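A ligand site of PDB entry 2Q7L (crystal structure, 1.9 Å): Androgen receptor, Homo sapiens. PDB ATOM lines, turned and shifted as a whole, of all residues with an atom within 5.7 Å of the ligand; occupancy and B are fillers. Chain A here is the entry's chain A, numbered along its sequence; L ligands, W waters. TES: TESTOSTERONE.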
ATOM      1  N   LEU A  39     -19.006  -5.485  -0.520  1.00  0.00           N
ATOM      2  CA  LEU A  39     -19.808  -5.600   0.704  1.00  0.00           C
ATOM      3  C   LEU A  39     -20.321  -7.022   0.891  1.00  0.00           C
ATOM      4  O   LEU A  39     -20.339  -7.524   2.020  1.00  0.00           O
ATOM      5  CB  LEU A  39     -20.955  -4.600   0.739  1.00  0.00           C
ATOM      6  CG  LEU A  39     -20.674  -3.302   1.495  1.00  0.00           C
ATOM      7  CD1 LEU A  39     -20.462  -3.539   2.983  1.00  0.00           C
ATOM      8  CD2 LEU A  39     -19.488  -2.510   0.891  1.00  0.00           C
ATOM      9  N   LEU A  42     -17.376  -8.810   2.333  1.00  0.00           N
ATOM     10  CA  LEU A  42     -17.233  -8.470   3.737  1.00  0.00           C
ATOM     11  C   LEU A  42     -18.250  -9.208   4.618  1.00  0.00           C
ATOM     12  O   LEU A  42     -17.898  -9.637   5.715  1.00  0.00           O
ATOM     13  CB  LEU A  42     -17.341  -6.953   3.953  1.00  0.00           C
ATOM     14  CG  LEU A  42     -16.098  -6.124   3.552  1.00  0.00           C
ATOM     15  CD1 LEU A  42     -16.393  -4.653   3.619  1.00  0.00           C
ATOM     16  CD2 LEU A  42     -14.882  -6.467   4.420  1.00  0.00           C
ATOM     17  N   ASN A  43     -19.496  -9.326   4.146  1.00  0.00           N
ATOM     18  CA  ASN A  43     -20.576  -9.971   4.890  1.00  0.00           C
ATOM     19  C   ASN A  43     -20.309 -11.471   5.038  1.00  0.00           C
ATOM     20  O   ASN A  43     -20.487 -12.052   6.111  1.00  0.00           O
ATOM     21  CB  ASN A  43     -21.938  -9.739   4.210  1.00  0.00           C
ATOM     22  CG  ASN A  43     -22.467  -8.338   4.415  1.00  0.00           C
ATOM     23  OD1 ASN A  43     -22.016  -7.623   5.308  1.00  0.00           O
ATOM     24  ND2 ASN A  43     -23.449  -7.947   3.594  1.00  0.00           N
ATOM     25  N   LEU A  45     -17.252 -12.785   4.926  1.00  0.00           N
ATOM     26  CA  LEU A  45     -16.128 -12.850   5.846  1.00  0.00           C
ATOM     27  C   LEU A  45     -16.599 -12.763   7.288  1.00  0.00           C
ATOM     28  O   LEU A  45     -16.107 -13.486   8.146  1.00  0.00           O
ATOM     29  CB  LEU A  45     -15.126 -11.716   5.552  1.00  0.00           C
ATOM     30  CG  LEU A  45     -13.879 -11.700   6.447  1.00  0.00           C
ATOM     31  CD1 LEU A  45     -13.064 -12.951   6.259  1.00  0.00           C
ATOM     32  CD2 LEU A  45     -13.038 -10.463   6.154  1.00  0.00           C
ATOM     33  N   GLY A  46     -17.566 -11.868   7.542  1.00  0.00           N
ATOM     34  CA  GLY A  46     -18.149 -11.740   8.856  1.00  0.00           C
ATOM     35  C   GLY A  46     -18.737 -13.053   9.352  1.00  0.00           C
ATOM     36  O   GLY A  46     -18.521 -13.418  10.506  1.00  0.00           O
ATOM     37  N   GLN A  49     -15.860 -15.493  10.084  1.00  0.00           N
ATOM     38  CA  GLN A  49     -15.142 -15.138  11.305  1.00  0.00           C
ATOM     39  C   GLN A  49     -16.005 -15.391  12.533  1.00  0.00           C
ATOM     40  O   GLN A  49     -15.469 -15.743  13.584  1.00  0.00           O
ATOM     41  CB  GLN A  49     -14.631 -13.691  11.268  1.00  0.00           C
ATOM     42  CG  GLN A  49     -13.471 -13.473  10.328  1.00  0.00           C
ATOM     43  CD  GLN A  49     -12.773 -12.141  10.512  1.00  0.00           C
ATOM     44  OE1 GLN A  49     -11.911 -11.762   9.707  1.00  0.00           O
ATOM     45  NE2 GLN A  49     -13.132 -11.423  11.569  1.00  0.00           N
ATOM     46  N   TRP A  79     -19.051  -8.895  18.720  1.00  0.00           N
ATOM     47  CA  TRP A  79     -18.354  -9.384  17.521  1.00  0.00           C
ATOM     48  C   TRP A  79     -17.749  -8.282  16.643  1.00  0.00           C
ATOM     49  O   TRP A  79     -16.618  -8.439  16.188  1.00  0.00           O
ATOM     50  CB  TRP A  79     -19.233 -10.294  16.660  1.00  0.00           C
ATOM     51  CG  TRP A  79     -20.463  -9.652  16.120  1.00  0.00           C
ATOM     52  CD1 TRP A  79     -21.660  -9.519  16.752  1.00  0.00           C
ATOM     53  CD2 TRP A  79     -20.650  -9.085  14.817  1.00  0.00           C
ATOM     54  NE1 TRP A  79     -22.579  -8.912  15.936  1.00  0.00           N
ATOM     55  CE2 TRP A  79     -21.982  -8.624  14.735  1.00  0.00           C
ATOM     56  CE3 TRP A  79     -19.812  -8.907  13.703  1.00  0.00           C
ATOM     57  CZ2 TRP A  79     -22.494  -8.005  13.594  1.00  0.00           C
ATOM     58  CZ3 TRP A  79     -20.316  -8.306  12.573  1.00  0.00           C
ATOM     59  CH2 TRP A  79     -21.660  -7.852  12.518  1.00  0.00           C
ATOM     60  N   MET A  80     -18.467  -7.184  16.408  1.00  0.00           N
ATOM     61  CA  MET A  80     -17.929  -6.120  15.569  1.00  0.00           C
ATOM     62  C   MET A  80     -16.629  -5.579  16.150  1.00  0.00           C
ATOM     63  O   MET A  80     -15.631  -5.467  15.438  1.00  0.00           O
ATOM     64  CB  MET A  80     -18.922  -4.977  15.406  1.00  0.00           C
ATOM     65  CG  MET A  80     -18.491  -3.908  14.410  1.00  0.00           C
ATOM     66  SD  MET A  80     -18.557  -4.455  12.707  1.00  0.00           S
ATOM     67  CE  MET A  80     -20.342  -4.417  12.455  1.00  0.00           C
ATOM     68  N   MET A  83     -13.776  -8.085  15.925  1.00  0.00           N
ATOM     69  CA  MET A  83     -13.330  -8.315  14.549  1.00  0.00           C
ATOM     70  C   MET A  83     -12.576  -7.119  13.995  1.00  0.00           C
ATOM     71  O   MET A  83     -11.566  -7.275  13.320  1.00  0.00           O
ATOM     72  CB  MET A  83     -14.509  -8.684  13.673  1.00  0.00           C
ATOM     73  CG  MET A  83     -15.038 -10.107  13.998  1.00  0.00           C
ATOM     74  SD  MET A  83     -16.384 -10.561  12.926  1.00  0.00           S
ATOM     75  CE  MET A  83     -16.920 -12.091  13.692  1.00  0.00           C
ATOM     76  N   VAL A  84     -13.041  -5.922  14.344  1.00  0.00           N
ATOM     77  CA  VAL A  84     -12.334  -4.697  13.956  1.00  0.00           C
ATOM     78  C   VAL A  84     -10.953  -4.626  14.575  1.00  0.00           C
ATOM     79  O   VAL A  84      -9.975  -4.323  13.891  1.00  0.00           O
ATOM     80  CB  VAL A  84     -13.157  -3.450  14.318  1.00  0.00           C
ATOM     81  CG1 VAL A  84     -12.316  -2.162  14.162  1.00  0.00           C
ATOM     82  CG2 VAL A  84     -14.358  -3.366  13.425  1.00  0.00           C
ATOM     83  N   MET A  87      -8.663  -7.115  12.922  1.00  0.00           N
ATOM     84  CA  MET A  87      -8.321  -6.684  11.568  1.00  0.00           C
ATOM     85  C   MET A  87      -7.289  -5.573  11.617  1.00  0.00           C
ATOM     86  O   MET A  87      -6.350  -5.567  10.818  1.00  0.00           O
ATOM     87  CB  MET A  87      -9.583  -6.240  10.818  1.00  0.00           C
ATOM     88  CG  MET A  87      -9.348  -5.891   9.351  1.00  0.00           C
ATOM     89  SD  MET A  87      -8.792  -4.184   9.110  1.00  0.00           S
ATOM     90  CE  MET A  87     -10.260  -3.254   9.615  1.00  0.00           C
ATOM     91  N   ARG A  90      -3.954  -7.404  12.267  1.00  0.00           N
ATOM     92  CA  ARG A  90      -3.503  -7.978  10.996  1.00  0.00           C
ATOM     93  C   ARG A  90      -2.928  -6.918  10.060  1.00  0.00           C
ATOM     94  O   ARG A  90      -1.889  -7.125   9.429  1.00  0.00           O
ATOM     95  CB  ARG A  90      -4.655  -8.670  10.272  1.00  0.00           C
ATOM     96  CG  ARG A  90      -5.143  -9.929  10.927  1.00  0.00           C
ATOM     97  CD  ARG A  90      -5.987 -10.744   9.959  1.00  0.00           C
ATOM     98  NE  ARG A  90      -7.234 -10.088   9.583  1.00  0.00           N
ATOM     99  CZ  ARG A  90      -8.337 -10.061  10.342  1.00  0.00           C
ATOM    100  NH1 ARG A  90      -8.352 -10.631  11.534  1.00  0.00           N
ATOM    101  NH2 ARG A  90      -9.436  -9.462   9.882  1.00  0.00           N
ATOM    102  N   TYR A 101      -6.302  -5.030   6.070  1.00  0.00           N
ATOM    103  CA  TYR A 101      -6.109  -6.438   5.761  1.00  0.00           C
ATOM    104  C   TYR A 101      -7.283  -7.223   6.338  1.00  0.00           C
ATOM    105  O   TYR A 101      -7.154  -7.912   7.350  1.00  0.00           O
ATOM    106  CB  TYR A 101      -4.789  -6.912   6.372  1.00  0.00           C
ATOM    107  CG  TYR A 101      -4.257  -8.215   5.813  1.00  0.00           C
ATOM    108  CD1 TYR A 101      -3.216  -8.230   4.884  1.00  0.00           C
ATOM    109  CD2 TYR A 101      -4.766  -9.447   6.240  1.00  0.00           C
ATOM    110  CE1 TYR A 101      -2.715  -9.437   4.381  1.00  0.00           C
ATOM    111  CE2 TYR A 101      -4.268 -10.643   5.749  1.00  0.00           C
ATOM    112  CZ  TYR A 101      -3.243 -10.630   4.832  1.00  0.00           C
ATOM    113  OH  TYR A 101      -2.757 -11.833   4.368  1.00  0.00           O
ATOM    114  N   PHE A 102      -8.439  -7.109   5.673  1.00  0.00           N
ATOM    115  CA  PHE A 102      -9.644  -7.812   6.146  1.00  0.00           C
ATOM    116  C   PHE A 102      -9.382  -9.322   6.088  1.00  0.00           C
ATOM    117  O   PHE A 102      -9.710 -10.074   7.008  1.00  0.00           O
ATOM    118  CB  PHE A 102     -10.874  -7.438   5.324  1.00  0.00           C
ATOM    119  CG  PHE A 102     -11.410  -6.036   5.605  1.00  0.00           C
ATOM    120  CD1 PHE A 102     -12.182  -5.791   6.743  1.00  0.00           C
ATOM    121  CD2 PHE A 102     -11.153  -4.990   4.751  1.00  0.00           C
ATOM    122  CE1 PHE A 102     -12.685  -4.531   7.001  1.00  0.00           C
ATOM    123  CE2 PHE A 102     -11.636  -3.699   5.027  1.00  0.00           C
ATOM    124  CZ  PHE A 102     -12.418  -3.477   6.143  1.00  0.00           C
ATOM    125  N   MET A 118     -17.660   3.301   2.798  1.00  0.00           N
ATOM    126  CA  MET A 118     -17.340   3.310   4.228  1.00  0.00           C
ATOM    127  C   MET A 118     -15.995   3.981   4.436  1.00  0.00           C
ATOM    128  O   MET A 118     -15.230   3.590   5.319  1.00  0.00           O
ATOM    129  CB  MET A 118     -17.212   1.877   4.770  1.00  0.00           C
ATOM    130  CG  MET A 118     -18.423   1.022   4.618  1.00  0.00           C
ATOM    131  SD  MET A 118     -18.223  -0.465   5.637  1.00  0.00           S
ATOM    132  CE  MET A 118     -17.132  -1.431   4.634  1.00  0.00           C
ATOM    133  N   MET A 125     -10.520   2.952  11.228  1.00  0.00           N
ATOM    134  CA  MET A 125      -9.925   1.626  11.430  1.00  0.00           C
ATOM    135  C   MET A 125      -8.441   1.629  11.080  1.00  0.00           C
ATOM    136  O   MET A 125      -7.647   0.948  11.734  1.00  0.00           O
ATOM    137  CB  MET A 125     -10.680   0.575  10.609  1.00  0.00           C
ATOM    138  CG  MET A 125     -12.075   0.300  11.130  1.00  0.00           C
ATOM    139  SD  MET A 125     -12.891  -1.115  10.358  1.00  0.00           S
ATOM    140  CE  MET A 125     -13.399  -0.416   8.792  1.00  0.00           C
ATOM    141  N   LEU A 211     -20.009   1.249  12.352  1.00  0.00           N
ATOM    142  CA  LEU A 211     -20.136   0.088  11.474  1.00  0.00           C
ATOM    143  C   LEU A 211     -21.471  -0.638  11.705  1.00  0.00           C
ATOM    144  O   LEU A 211     -22.100  -1.128  10.769  1.00  0.00           O
ATOM    145  CB  LEU A 211     -18.950  -0.860  11.694  1.00  0.00           C
ATOM    146  CG  LEU A 211     -17.589  -0.326  11.224  1.00  0.00           C
ATOM    147  CD1 LEU A 211     -16.461  -1.192  11.718  1.00  0.00           C
ATOM    148  CD2 LEU A 211     -17.547  -0.210   9.704  1.00  0.00           C
ATOM    149  N   PHE A 214     -24.027   1.407   9.848  1.00  0.00           N
ATOM    150  CA  PHE A 214     -23.878   1.180   8.409  1.00  0.00           C
ATOM    151  C   PHE A 214     -24.463  -0.153   7.939  1.00  0.00           C
ATOM    152  O   PHE A 214     -25.190  -0.215   6.934  1.00  0.00           O
ATOM    153  CB  PHE A 214     -22.392   1.258   8.024  1.00  0.00           C
ATOM    154  CG  PHE A 214     -22.136   1.227   6.548  1.00  0.00           C
ATOM    155  CD1 PHE A 214     -21.898   0.029   5.898  1.00  0.00           C
ATOM    156  CD2 PHE A 214     -22.114   2.405   5.816  1.00  0.00           C
ATOM    157  CE1 PHE A 214     -21.650   0.001   4.521  1.00  0.00           C
ATOM    158  CE2 PHE A 214     -21.872   2.384   4.438  1.00  0.00           C
ATOM    159  CZ  PHE A 214     -21.635   1.186   3.788  1.00  0.00           C
ATOM    160  N   THR A 215     -24.144  -1.228   8.666  1.00  0.00           N
ATOM    161  CA  THR A 215     -24.599  -2.544   8.245  1.00  0.00           C
ATOM    162  C   THR A 215     -26.090  -2.703   8.473  1.00  0.00           C
ATOM    163  O   THR A 215     -26.763  -3.354   7.701  1.00  0.00           O
ATOM    164  CB  THR A 215     -23.789  -3.684   8.911  1.00  0.00           C
ATOM    165  OG1 THR A 215     -23.982  -4.886   8.163  1.00  0.00           O
ATOM    166  CG2 THR A 215     -24.196  -3.902  10.359  1.00  0.00           C
ATOM    167  N   LEU A 218     -27.687  -0.820   5.625  1.00  0.00           N
ATOM    168  CA  LEU A 218     -27.467  -1.658   4.443  1.00  0.00           C
ATOM    169  C   LEU A 218     -28.359  -2.896   4.456  1.00  0.00           C
ATOM    170  O   LEU A 218     -28.870  -3.289   3.417  1.00  0.00           O
ATOM    171  CB  LEU A 218     -25.990  -2.073   4.331  1.00  0.00           C
ATOM    172  CG  LEU A 218     -25.610  -2.940   3.122  1.00  0.00           C
ATOM    173  CD1 LEU A 218     -26.049  -2.305   1.804  1.00  0.00           C
ATOM    174  CD2 LEU A 218     -24.118  -3.207   3.110  1.00  0.00           C
ATOM    175  N   PHE A 229     -26.490 -10.852   2.492  1.00  0.00           N
ATOM    176  CA  PHE A 229     -26.174 -11.092   3.891  1.00  0.00           C
ATOM    177  C   PHE A 229     -26.435 -12.559   4.199  1.00  0.00           C
ATOM    178  O   PHE A 229     -27.541 -13.027   4.012  1.00  0.00           O
ATOM    179  CB  PHE A 229     -27.067 -10.261   4.789  1.00  0.00           C
ATOM    180  CG  PHE A 229     -26.654  -8.827   4.897  1.00  0.00           C
ATOM    181  CD1 PHE A 229     -27.035  -7.898   3.937  1.00  0.00           C
ATOM    182  CD2 PHE A 229     -25.925  -8.385   5.988  1.00  0.00           C
ATOM    183  CE1 PHE A 229     -26.678  -6.559   4.053  1.00  0.00           C
ATOM    184  CE2 PHE A 229     -25.545  -7.068   6.097  1.00  0.00           C
ATOM    185  CZ  PHE A 229     -25.950  -6.144   5.137  1.00  0.00           C
ATOM    186  N   ILE A 237     -28.074  -8.897  12.852  1.00  0.00           N
ATOM    187  CA  ILE A 237     -28.142  -7.475  12.502  1.00  0.00           C
ATOM    188  C   ILE A 237     -29.580  -6.900  12.638  1.00  0.00           C
ATOM    189  O   ILE A 237     -29.750  -5.710  12.878  1.00  0.00           O
ATOM    190  CB  ILE A 237     -27.516  -7.195  11.109  1.00  0.00           C
ATOM    191  CG1 ILE A 237     -26.002  -7.440  11.146  1.00  0.00           C
ATOM    192  CG2 ILE A 237     -27.778  -5.730  10.663  1.00  0.00           C
ATOM    193  CD1 ILE A 237     -25.334  -7.596   9.784  1.00  0.00           C
HETATM  194  C1  TES L   1     -15.670  -8.629   8.779  1.00  0.00           C
HETATM  195  C2  TES L   1     -14.475  -9.205   9.511  1.00  0.00           C
HETATM  196  C3  TES L   1     -13.419  -8.146   9.614  1.00  0.00           C
HETATM  197  O3  TES L   1     -12.234  -8.443   9.550  1.00  0.00           O
HETATM  198  C4  TES L   1     -13.834  -6.723   9.773  1.00  0.00           C
HETATM  199  C5  TES L   1     -15.120  -6.364   9.708  1.00  0.00           C
HETATM  200  C6  TES L   1     -15.470  -4.908   9.949  1.00  0.00           C
HETATM  201  C7  TES L   1     -16.396  -4.423   8.829  1.00  0.00           C
HETATM  202  C8  TES L   1     -17.641  -5.306   8.790  1.00  0.00           C
HETATM  203  C9  TES L   1     -17.263  -6.761   8.460  1.00  0.00           C
HETATM  204  C10 TES L   1     -16.236  -7.369   9.447  1.00  0.00           C
HETATM  205  C11 TES L   1     -18.512  -7.648   8.273  1.00  0.00           C
HETATM  206  C12 TES L   1     -19.542  -7.080   7.275  1.00  0.00           C
HETATM  207  C13 TES L   1     -19.895  -5.643   7.611  1.00  0.00           C
HETATM  208  C14 TES L   1     -18.619  -4.805   7.730  1.00  0.00           C
HETATM  209  C15 TES L   1     -19.147  -3.377   7.808  1.00  0.00           C
HETATM  210  C16 TES L   1     -20.330  -3.388   6.831  1.00  0.00           C
HETATM  211  C17 TES L   1     -20.588  -4.860   6.489  1.00  0.00           C
HETATM  212  O17 TES L   1     -21.996  -5.154   6.338  1.00  0.00           O
HETATM  213  C18 TES L   1     -20.722  -5.646   8.885  1.00  0.00           C
HETATM  214  C19 TES L   1     -16.832  -7.679  10.834  1.00  0.00           C
HETATM  215  O   HOH W   1     -11.207  -9.797  12.363  1.00  0.00           O
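An oxygen (O17) of the ligand sits at hydrogen-bond distance from the side-chain hydroxyl of Thr 215 (2.7 Å). An oxygen (O3) of the ligand lies within hydrogen-bond range of the guanidinium group (NH2) of Arg 90, at 3.0 Å. The side-chain amide oxygen (OE1) of Gln 49 lies close to an oxygen (O3) of the ligand (3.3 Å). OD1 of Asn 43 sits at hydrogen-bond distance from O17 of the ligand.
NE of Arg 90 sits at hydrogen-bond distance from O of Tyr 101. The side-chain amide oxygen of Gln 49 lies within hydrogen-bond range of the guanidinium group of Arg 90 (3.4 Å). NE2 of Gln 49 lies close to SD of Met 83. The guanidinium group (NH2) of Arg 90 is in hydrogen-bond range of the backbone carbonyl oxygen (O) of Phe 102, at 3.0 Å.
Merely in contact with the ligand: Leu 42, Phe 102, Met 83, Met 87, Met 118, Leu 39, Met 80, Leu 45, Phe 214, Trp 79, Gly 46 and Val 84. Hydrophobic or aromatic side chains within 4 Å of the ligand: Leu 39, Leu 42, Leu 45, Trp 79, Met 80, Met 83, Val 84, Met 87, Phe 102, Met 118 and Phe 214. Of the 22 residues printed, 16 come within 4 Å of the ligand. Along chain A the residues within 4 Å of the ligand span positions 39 to 215. The nearest printed residue that does not touch the ligand is Leu 211 (4.02 Å).
Water W1 lies within hydrogen-bond range of the side-chain amide nitrogen (NE2) of Gln 49 (2.6 Å), the backbone carbonyl oxygen (O) of Met 83 (2.7 Å), the guanidinium group (NH2) of Arg 90 (3.1 Å) and an oxygen (O3) of the ligand (3.3 Å).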
